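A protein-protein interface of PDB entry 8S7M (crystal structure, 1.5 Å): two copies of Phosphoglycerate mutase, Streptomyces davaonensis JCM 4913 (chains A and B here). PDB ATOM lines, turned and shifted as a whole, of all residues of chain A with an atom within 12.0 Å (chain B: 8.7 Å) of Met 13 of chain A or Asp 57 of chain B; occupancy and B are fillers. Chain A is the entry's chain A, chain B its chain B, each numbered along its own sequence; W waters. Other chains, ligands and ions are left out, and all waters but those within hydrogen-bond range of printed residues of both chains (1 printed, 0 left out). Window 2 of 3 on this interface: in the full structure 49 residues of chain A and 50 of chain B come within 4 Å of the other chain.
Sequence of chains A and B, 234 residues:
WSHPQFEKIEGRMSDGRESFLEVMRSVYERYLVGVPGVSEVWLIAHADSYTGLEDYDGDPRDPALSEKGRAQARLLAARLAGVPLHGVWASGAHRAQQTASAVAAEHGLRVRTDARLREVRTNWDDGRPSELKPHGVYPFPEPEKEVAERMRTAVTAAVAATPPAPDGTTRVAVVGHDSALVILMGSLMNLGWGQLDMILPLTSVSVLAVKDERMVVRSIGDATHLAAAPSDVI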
ATOM      1  N   MET A  13     -24.059 -12.069  -3.903  1.00  0.00           N
ATOM      2  CA  MET A  13     -23.189 -11.140  -3.188  1.00  0.00           C
ATOM      3  C   MET A  13     -23.752  -9.713  -3.159  1.00  0.00           C
ATOM      4  O   MET A  13     -23.750  -9.067  -2.112  1.00  0.00           O
ATOM      5  CB  MET A  13     -21.779 -11.162  -3.782  1.00  0.00           C
ATOM      6  CG  MET A  13     -20.846 -12.169  -3.124  1.00  0.00           C
ATOM      7  SD  MET A  13     -20.958 -12.137  -1.323  1.00  0.00           S
ATOM      8  CE  MET A  13     -20.069 -13.634  -0.892  1.00  0.00           C
ATOM      9  N   SER A  14     -24.223  -9.226  -4.311  1.00  0.00           N
ATOM     10  CA  SER A  14     -24.903  -7.928  -4.400  1.00  0.00           C
ATOM     11  C   SER A  14     -26.418  -8.112  -4.284  1.00  0.00           C
ATOM     12  O   SER A  14     -27.214  -7.693  -5.126  1.00  0.00           O
ATOM     13  CB  SER A  14     -24.512  -7.210  -5.686  1.00  0.00           C
ATOM     14  OG  SER A  14     -24.668  -8.068  -6.802  1.00  0.00           O
ATOM     15  N   ASP A  15     -26.796  -8.752  -3.180  1.00  0.00           N
ATOM     16  CA  ASP A  15     -28.122  -9.311  -2.963  1.00  0.00           C
ATOM     17  C   ASP A  15     -28.986  -8.455  -2.040  1.00  0.00           C
ATOM     18  O   ASP A  15     -29.974  -8.958  -1.486  1.00  0.00           O
ATOM     19  CB  ASP A  15     -27.975 -10.723  -2.395  1.00  0.00           C
ATOM     20  CG  ASP A  15     -27.249 -10.759  -1.046  1.00  0.00           C
ATOM     21  OD1 ASP A  15     -26.925  -9.686  -0.469  1.00  0.00           O
ATOM     22  OD2 ASP A  15     -27.003 -11.878  -0.551  1.00  0.00           O
ATOM     23  N   GLY A  16     -28.633  -7.186  -1.863  1.00  0.00           N
ATOM     24  CA  GLY A  16     -29.281  -6.312  -0.900  1.00  0.00           C
ATOM     25  C   GLY A  16     -28.452  -6.048   0.339  1.00  0.00           C
ATOM     26  O   GLY A  16     -28.760  -5.103   1.084  1.00  0.00           O
ATOM     27  N   ARG A  17     -27.391  -6.825   0.580  1.00  0.00           N
ATOM     28  CA  ARG A  17     -26.608  -6.597   1.794  1.00  0.00           C
ATOM     29  C   ARG A  17     -25.818  -5.288   1.738  1.00  0.00           C
ATOM     30  O   ARG A  17     -25.544  -4.690   2.783  1.00  0.00           O
ATOM     31  CB  ARG A  17     -25.682  -7.773   2.104  1.00  0.00           C
ATOM     32  CG  ARG A  17     -24.492  -7.880   1.175  1.00  0.00           C
ATOM     33  CD  ARG A  17     -23.707  -9.141   1.480  1.00  0.00           C
ATOM     34  NE  ARG A  17     -24.428 -10.350   1.103  1.00  0.00           N
ATOM     35  CZ  ARG A  17     -23.969 -11.584   1.301  1.00  0.00           C
ATOM     36  NH1 ARG A  17     -22.837 -11.810   1.956  1.00  0.00           N
ATOM     37  NH2 ARG A  17     -24.667 -12.617   0.837  1.00  0.00           N
ATOM     38  N   GLU A  18     -25.449  -4.817   0.550  1.00  0.00           N
ATOM     39  CA  GLU A  18     -24.640  -3.600   0.505  1.00  0.00           C
ATOM     40  C   GLU A  18     -25.447  -2.367   0.899  1.00  0.00           C
ATOM     41  O   GLU A  18     -24.955  -1.508   1.648  1.00  0.00           O
ATOM     42  CB  GLU A  18     -24.005  -3.433  -0.872  1.00  0.00           C
ATOM     43  CG  GLU A  18     -22.988  -4.527  -1.216  1.00  0.00           C
ATOM     44  CD  GLU A  18     -21.744  -4.440  -0.345  1.00  0.00           C
ATOM     45  OE1 GLU A  18     -21.556  -3.385   0.302  1.00  0.00           O
ATOM     46  OE2 GLU A  18     -20.959  -5.418  -0.311  1.00  0.00           O
ATOM     47  N   SER A  19     -26.682  -2.252   0.407  1.00  0.00           N
ATOM     48  CA  SER A  19     -27.514  -1.115   0.806  1.00  0.00           C
ATOM     49  C   SER A  19     -27.885  -1.206   2.280  1.00  0.00           C
ATOM     50  O   SER A  19     -27.938  -0.183   2.981  1.00  0.00           O
ATOM     51  CB  SER A  19     -28.763  -1.049  -0.076  1.00  0.00           C
ATOM     52  OG  SER A  19     -29.605  -2.153   0.191  1.00  0.00           O
ATOM     53  N   PHE A  20     -28.147  -2.425   2.764  1.00  0.00           N
ATOM     54  CA  PHE A  20     -28.409  -2.646   4.181  1.00  0.00           C
ATOM     55  C   PHE A  20     -27.263  -2.131   5.036  1.00  0.00           C
ATOM     56  O   PHE A  20     -27.486  -1.387   5.998  1.00  0.00           O
ATOM     57  CB  PHE A  20     -28.667  -4.135   4.421  1.00  0.00           C
ATOM     58  CG  PHE A  20     -28.799  -4.517   5.875  1.00  0.00           C
ATOM     59  CD1 PHE A  20     -29.937  -4.199   6.600  1.00  0.00           C
ATOM     60  CD2 PHE A  20     -27.804  -5.255   6.487  1.00  0.00           C
ATOM     61  CE1 PHE A  20     -30.047  -4.573   7.924  1.00  0.00           C
ATOM     62  CE2 PHE A  20     -27.909  -5.636   7.810  1.00  0.00           C
ATOM     63  CZ  PHE A  20     -29.027  -5.298   8.531  1.00  0.00           C
ATOM     64  N   LEU A  21     -26.026  -2.475   4.671  1.00  0.00           N
ATOM     65  CA  LEU A  21     -24.869  -2.052   5.462  1.00  0.00           C
ATOM     66  C   LEU A  21     -24.627  -0.553   5.339  1.00  0.00           C
ATOM     67  O   LEU A  21     -24.237   0.102   6.317  1.00  0.00           O
ATOM     68  CB  LEU A  21     -23.632  -2.832   5.042  1.00  0.00           C
ATOM     69  CG  LEU A  21     -23.573  -4.319   5.389  1.00  0.00           C
ATOM     70  CD1 LEU A  21     -22.470  -4.976   4.568  1.00  0.00           C
ATOM     71  CD2 LEU A  21     -23.366  -4.558   6.895  1.00  0.00           C
ATOM     72  N   GLU A  22     -24.831   0.007   4.149  1.00  0.00           N
ATOM     73  CA  GLU A  22     -24.568   1.425   3.969  1.00  0.00           C
ATOM     74  C   GLU A  22     -25.545   2.251   4.797  1.00  0.00           C
ATOM     75  O   GLU A  22     -25.147   3.198   5.493  1.00  0.00           O
ATOM     76  CB  GLU A  22     -24.650   1.785   2.486  1.00  0.00           C
ATOM     77  CG  GLU A  22     -24.362   3.238   2.165  1.00  0.00           C
ATOM     78  CD  GLU A  22     -22.900   3.625   2.344  1.00  0.00           C
ATOM     79  OE1 GLU A  22     -22.082   2.767   2.750  1.00  0.00           O
ATOM     80  OE2 GLU A  22     -22.572   4.799   2.063  1.00  0.00           O
ATOM     81  N   ARG A  25     -24.547   2.000   8.537  1.00  0.00           N
ATOM     82  CA  ARG A  25     -23.448   2.893   8.881  1.00  0.00           C
ATOM     83  C   ARG A  25     -23.919   4.337   8.985  1.00  0.00           C
ATOM     84  O   ARG A  25     -23.512   5.053   9.903  1.00  0.00           O
ATOM     85  CB  ARG A  25     -22.308   2.786   7.868  1.00  0.00           C
ATOM     86  CG  ARG A  25     -21.677   1.425   7.791  1.00  0.00           C
ATOM     87  CD  ARG A  25     -20.617   1.422   6.706  1.00  0.00           C
ATOM     88  NE  ARG A  25     -20.138   0.082   6.402  1.00  0.00           N
ATOM     89  CZ  ARG A  25     -20.224  -0.477   5.203  1.00  0.00           C
ATOM     90  NH1 ARG A  25     -20.767   0.166   4.180  1.00  0.00           N
ATOM     91  NH2 ARG A  25     -19.753  -1.709   5.026  1.00  0.00           N
ATOM     92  N   GLY B  52     -17.698  -7.678   8.245  1.00  0.00           N
ATOM     93  CA  GLY B  52     -17.395  -8.736   7.309  1.00  0.00           C
ATOM     94  C   GLY B  52     -18.586  -9.322   6.584  1.00  0.00           C
ATOM     95  O   GLY B  52     -18.409 -10.285   5.823  1.00  0.00           O
ATOM     96  N   LEU B  53     -19.789  -8.770   6.773  1.00  0.00           N
ATOM     97  CA  LEU B  53     -20.965  -9.351   6.130  1.00  0.00           C
ATOM     98  C   LEU B  53     -20.862  -9.292   4.617  1.00  0.00           C
ATOM     99  O   LEU B  53     -21.407 -10.162   3.926  1.00  0.00           O
ATOM    100  CB  LEU B  53     -22.234  -8.629   6.572  1.00  0.00           C
ATOM    101  CG  LEU B  53     -23.559  -9.290   6.176  1.00  0.00           C
ATOM    102  CD1 LEU B  53     -23.730 -10.618   6.930  1.00  0.00           C
ATOM    103  CD2 LEU B  53     -24.748  -8.355   6.484  1.00  0.00           C
ATOM    104  N   GLU B  54     -20.159  -8.296   4.085  1.00  0.00           N
ATOM    105  CA  GLU B  54     -20.072  -8.174   2.634  1.00  0.00           C
ATOM    106  C   GLU B  54     -19.454  -9.416   1.986  1.00  0.00           C
ATOM    107  O   GLU B  54     -19.748  -9.708   0.823  1.00  0.00           O
ATOM    108  CB  GLU B  54     -19.342  -6.882   2.238  1.00  0.00           C
ATOM    109  CG  GLU B  54     -17.932  -6.742   2.782  1.00  0.00           C
ATOM    110  CD  GLU B  54     -17.878  -6.290   4.240  1.00  0.00           C
ATOM    111  OE1 GLU B  54     -16.751  -6.231   4.788  1.00  0.00           O
ATOM    112  OE2 GLU B  54     -18.939  -5.987   4.828  1.00  0.00           O
ATOM    113  N   ASP B  55     -18.623 -10.167   2.716  1.00  0.00           N
ATOM    114  CA  ASP B  55     -17.950 -11.343   2.163  1.00  0.00           C
ATOM    115  C   ASP B  55     -18.447 -12.668   2.743  1.00  0.00           C
ATOM    116  O   ASP B  55     -17.830 -13.711   2.496  1.00  0.00           O
ATOM    117  CB  ASP B  55     -16.439 -11.242   2.364  1.00  0.00           C
ATOM    118  CG  ASP B  55     -15.835 -10.027   1.691  1.00  0.00           C
ATOM    119  OD1 ASP B  55     -16.224  -9.720   0.543  1.00  0.00           O
ATOM    120  OD2 ASP B  55     -14.956  -9.390   2.310  1.00  0.00           O
ATOM    121  N   TYR B  56     -19.532 -12.655   3.503  1.00  0.00           N
ATOM    122  CA  TYR B  56     -19.994 -13.826   4.236  1.00  0.00           C
ATOM    123  C   TYR B  56     -20.716 -14.777   3.288  1.00  0.00           C
ATOM    124  O   TYR B  56     -21.528 -14.350   2.462  1.00  0.00           O
ATOM    125  CB  TYR B  56     -20.980 -13.337   5.287  1.00  0.00           C
ATOM    126  CG  TYR B  56     -21.467 -14.333   6.305  1.00  0.00           C
ATOM    127  CD1 TYR B  56     -20.585 -14.977   7.163  1.00  0.00           C
ATOM    128  CD2 TYR B  56     -22.819 -14.588   6.451  1.00  0.00           C
ATOM    129  CE1 TYR B  56     -21.046 -15.853   8.133  1.00  0.00           C
ATOM    130  CE2 TYR B  56     -23.287 -15.459   7.407  1.00  0.00           C
ATOM    131  CZ  TYR B  56     -22.405 -16.080   8.252  1.00  0.00           C
ATOM    132  OH  TYR B  56     -22.881 -16.942   9.224  1.00  0.00           O
ATOM    133  N   ASP B  57     -20.436 -16.079   3.418  1.00  0.00           N
ATOM    134  CA  ASP B  57     -21.046 -17.082   2.549  1.00  0.00           C
ATOM    135  C   ASP B  57     -22.174 -17.865   3.213  1.00  0.00           C
ATOM    136  O   ASP B  57     -22.804 -18.701   2.550  1.00  0.00           O
ATOM    137  CB  ASP B  57     -19.990 -18.020   1.953  1.00  0.00           C
ATOM    138  CG  ASP B  57     -19.350 -17.439   0.711  1.00  0.00           C
ATOM    139  OD1 ASP B  57     -20.063 -16.738  -0.044  1.00  0.00           O
ATOM    140  OD2 ASP B  57     -18.138 -17.654   0.504  1.00  0.00           O
ATOM    141  N   GLY B  58     -22.420 -17.635   4.494  1.00  0.00           N
ATOM    142  CA  GLY B  58     -23.600 -18.147   5.163  1.00  0.00           C
ATOM    143  C   GLY B  58     -24.845 -17.353   4.795  1.00  0.00           C
ATOM    144  O   GLY B  58     -24.871 -16.570   3.843  1.00  0.00           O
ATOM    145  N   ASP B  59     -25.899 -17.593   5.554  1.00  0.00           N
ATOM    146  CA  ASP B  59     -27.150 -16.880   5.342  1.00  0.00           C
ATOM    147  C   ASP B  59     -26.941 -15.444   5.814  1.00  0.00           C
ATOM    148  O   ASP B  59     -26.784 -15.224   7.017  1.00  0.00           O
ATOM    149  CB  ASP B  59     -28.247 -17.579   6.145  1.00  0.00           C
ATOM    150  CG  ASP B  59     -29.609 -16.936   5.980  1.00  0.00           C
ATOM    151  OD1 ASP B  59     -29.700 -15.812   5.430  1.00  0.00           O
ATOM    152  OD2 ASP B  59     -30.599 -17.593   6.363  1.00  0.00           O
ATOM    153  N   PRO B  60     -26.902 -14.452   4.912  1.00  0.00           N
ATOM    154  CA  PRO B  60     -26.539 -13.087   5.333  1.00  0.00           C
ATOM    155  C   PRO B  60     -27.611 -12.402   6.154  1.00  0.00           C
ATOM    156  O   PRO B  60     -27.316 -11.396   6.810  1.00  0.00           O
ATOM    157  CB  PRO B  60     -26.346 -12.359   4.001  1.00  0.00           C
ATOM    158  CG  PRO B  60     -27.304 -13.053   3.081  1.00  0.00           C
ATOM    159  CD  PRO B  60     -27.336 -14.501   3.507  1.00  0.00           C
ATOM    160  N   PRO B  63     -26.757 -14.161  10.179  1.00  0.00           N
ATOM    161  CA  PRO B  63     -25.332 -14.446  10.366  1.00  0.00           C
ATOM    162  C   PRO B  63     -24.973 -14.794  11.806  1.00  0.00           C
ATOM    163  O   PRO B  63     -25.630 -14.375  12.765  1.00  0.00           O
ATOM    164  CB  PRO B  63     -24.668 -13.118   9.984  1.00  0.00           C
ATOM    165  CG  PRO B  63     -25.660 -12.097  10.370  1.00  0.00           C
ATOM    166  CD  PRO B  63     -27.005 -12.704  10.051  1.00  0.00           C
ATOM    167  N   TRP B 124     -34.646  -5.360   3.734  1.00  0.00           N
ATOM    168  CA  TRP B 124     -33.659  -6.420   3.499  1.00  0.00           C
ATOM    169  C   TRP B 124     -34.289  -7.811   3.617  1.00  0.00           C
ATOM    170  O   TRP B 124     -34.116  -8.664   2.732  1.00  0.00           O
ATOM    171  CB  TRP B 124     -32.533  -6.180   4.523  1.00  0.00           C
ATOM    172  CG  TRP B 124     -31.336  -7.122   4.676  1.00  0.00           C
ATOM    173  CD1 TRP B 124     -30.707  -7.433   5.851  1.00  0.00           C
ATOM    174  CD2 TRP B 124     -30.626  -7.828   3.653  1.00  0.00           C
ATOM    175  NE1 TRP B 124     -29.662  -8.290   5.626  1.00  0.00           N
ATOM    176  CE2 TRP B 124     -29.591  -8.551   4.285  1.00  0.00           C
ATOM    177  CE3 TRP B 124     -30.768  -7.928   2.270  1.00  0.00           C
ATOM    178  CZ2 TRP B 124     -28.706  -9.357   3.578  1.00  0.00           C
ATOM    179  CZ3 TRP B 124     -29.902  -8.721   1.582  1.00  0.00           C
ATOM    180  CH2 TRP B 124     -28.878  -9.427   2.230  1.00  0.00           C
HETATM  181  O   HOH W   1     -24.151 -15.412   1.430  1.00  0.00           O
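The side-chain sulfur (SD) of Met 13 of chain A lies close to the backbone carbonyl oxygen (O) of Glu 54 of chain B (3.5 Å). The backbone carbonyl oxygen (O) of Leu 53 of chain B is in hydrogen-bond range of the guanidinium group (NH1) of Arg 17 of chain A, 2.9 Å away. O of Tyr 56 of chain B sits at hydrogen-bond distance from NH1 of Arg 17 of chain A, 2.9 Å away.
NH2 of Arg 17 of chain A lies within salt-bridge range of OD2 of Asp 15 of chain A, at 2.8 Å. O of Gly 16 of chain A is in hydrogen-bond range of OG of Ser 19 of chain A (3.2 Å). SD of Met 13 of chain A is in hydrogen-bond range of NH1 of Arg 17 of chain A, 3.8 Å away.
Among the printed residues, pairs that only touch across the chains: Met 13 of chain A with Tyr 56 of chain B (3.7 Å), Met 13 of chain A with Asp 57 of chain B (3.2 Å), Asp 15 of chain A with Pro 60 of chain B (3.8 Å), Asp 15 of chain A with Trp 124 of chain B (3.1 Å), Gly 16 of chain A with Trp 124 of chain B (3.3 Å), Arg 17 of chain A with Glu 54 of chain B (3.9 Å), Arg 17 of chain A with Pro 60 of chain B (3.5 Å), Arg 17 of chain A with Trp 124 of chain B (3.3 Å), Glu 18 of chain A with Glu 54 of chain B (3.4 Å), Phe 20 of chain A with Trp 124 of chain B (3.4 Å) and Leu 21 of chain A with Glu 54 of chain B (3.7 Å).
Of chain B, only Glu 54 (3.5 Å), Tyr 56 (3.7 Å) and Asp 57 (3.2 Å) come within 4 Å of Met 13 of chain A. Of chain A, only Met 13 comes within 4 Å of Asp 57 of chain B. Ser 14 of chain A touches none of the printed residues of chain B. No residue of chain A comes within 4 Å of Asp 55 of chain B. Of chain A, only Met 13 and Arg 17 come within 4 Å of Tyr 56 of chain B. Of the printed residues of chain A, Trp 124 of chain B touches Asp 15 (3.1 Å), Gly 16 (3.3 Å), Arg 17 (3.3 Å) and Phe 20 (3.4 Å). Of the printed residues of chain A, Glu 54 of chain B touches Met 13, Arg 17, Glu 18 and Leu 21. Printed residues of chain B within 4 Å of Leu 21 of chain A: Glu 54. The nearest residue of chain A that does not touch Asp 57 of chain B is Arg 17 of chain A (5.1 Å). The nearest printed residue of chain A that does not touch Leu 53 of chain B is Leu 21 of chain A (4.1 Å).
Hydrophobic or aromatic side chains of chain B within 4 Å of the printed part of chain A: Pro 60 and Trp 124. Among the printed residues, no Asp or Glu carboxylate lies within 4 Å of a Lys or Arg side-chain nitrogen of the other chain.
No position is printed for both chains. Of the 14 pairs that touch across the chains among the printed residues, none has its exchanged pair printed and touching as well.
Water W1 lies within hydrogen-bond range of the backbone carbonyl oxygen (O) of Gly 58 of chain B (2.8 Å), the guanidinium group (NH2) of Arg 17 of chain A (2.9 Å) and the backbone carbonyl oxygen (O) of Tyr 56 of chain B (3.0 Å).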
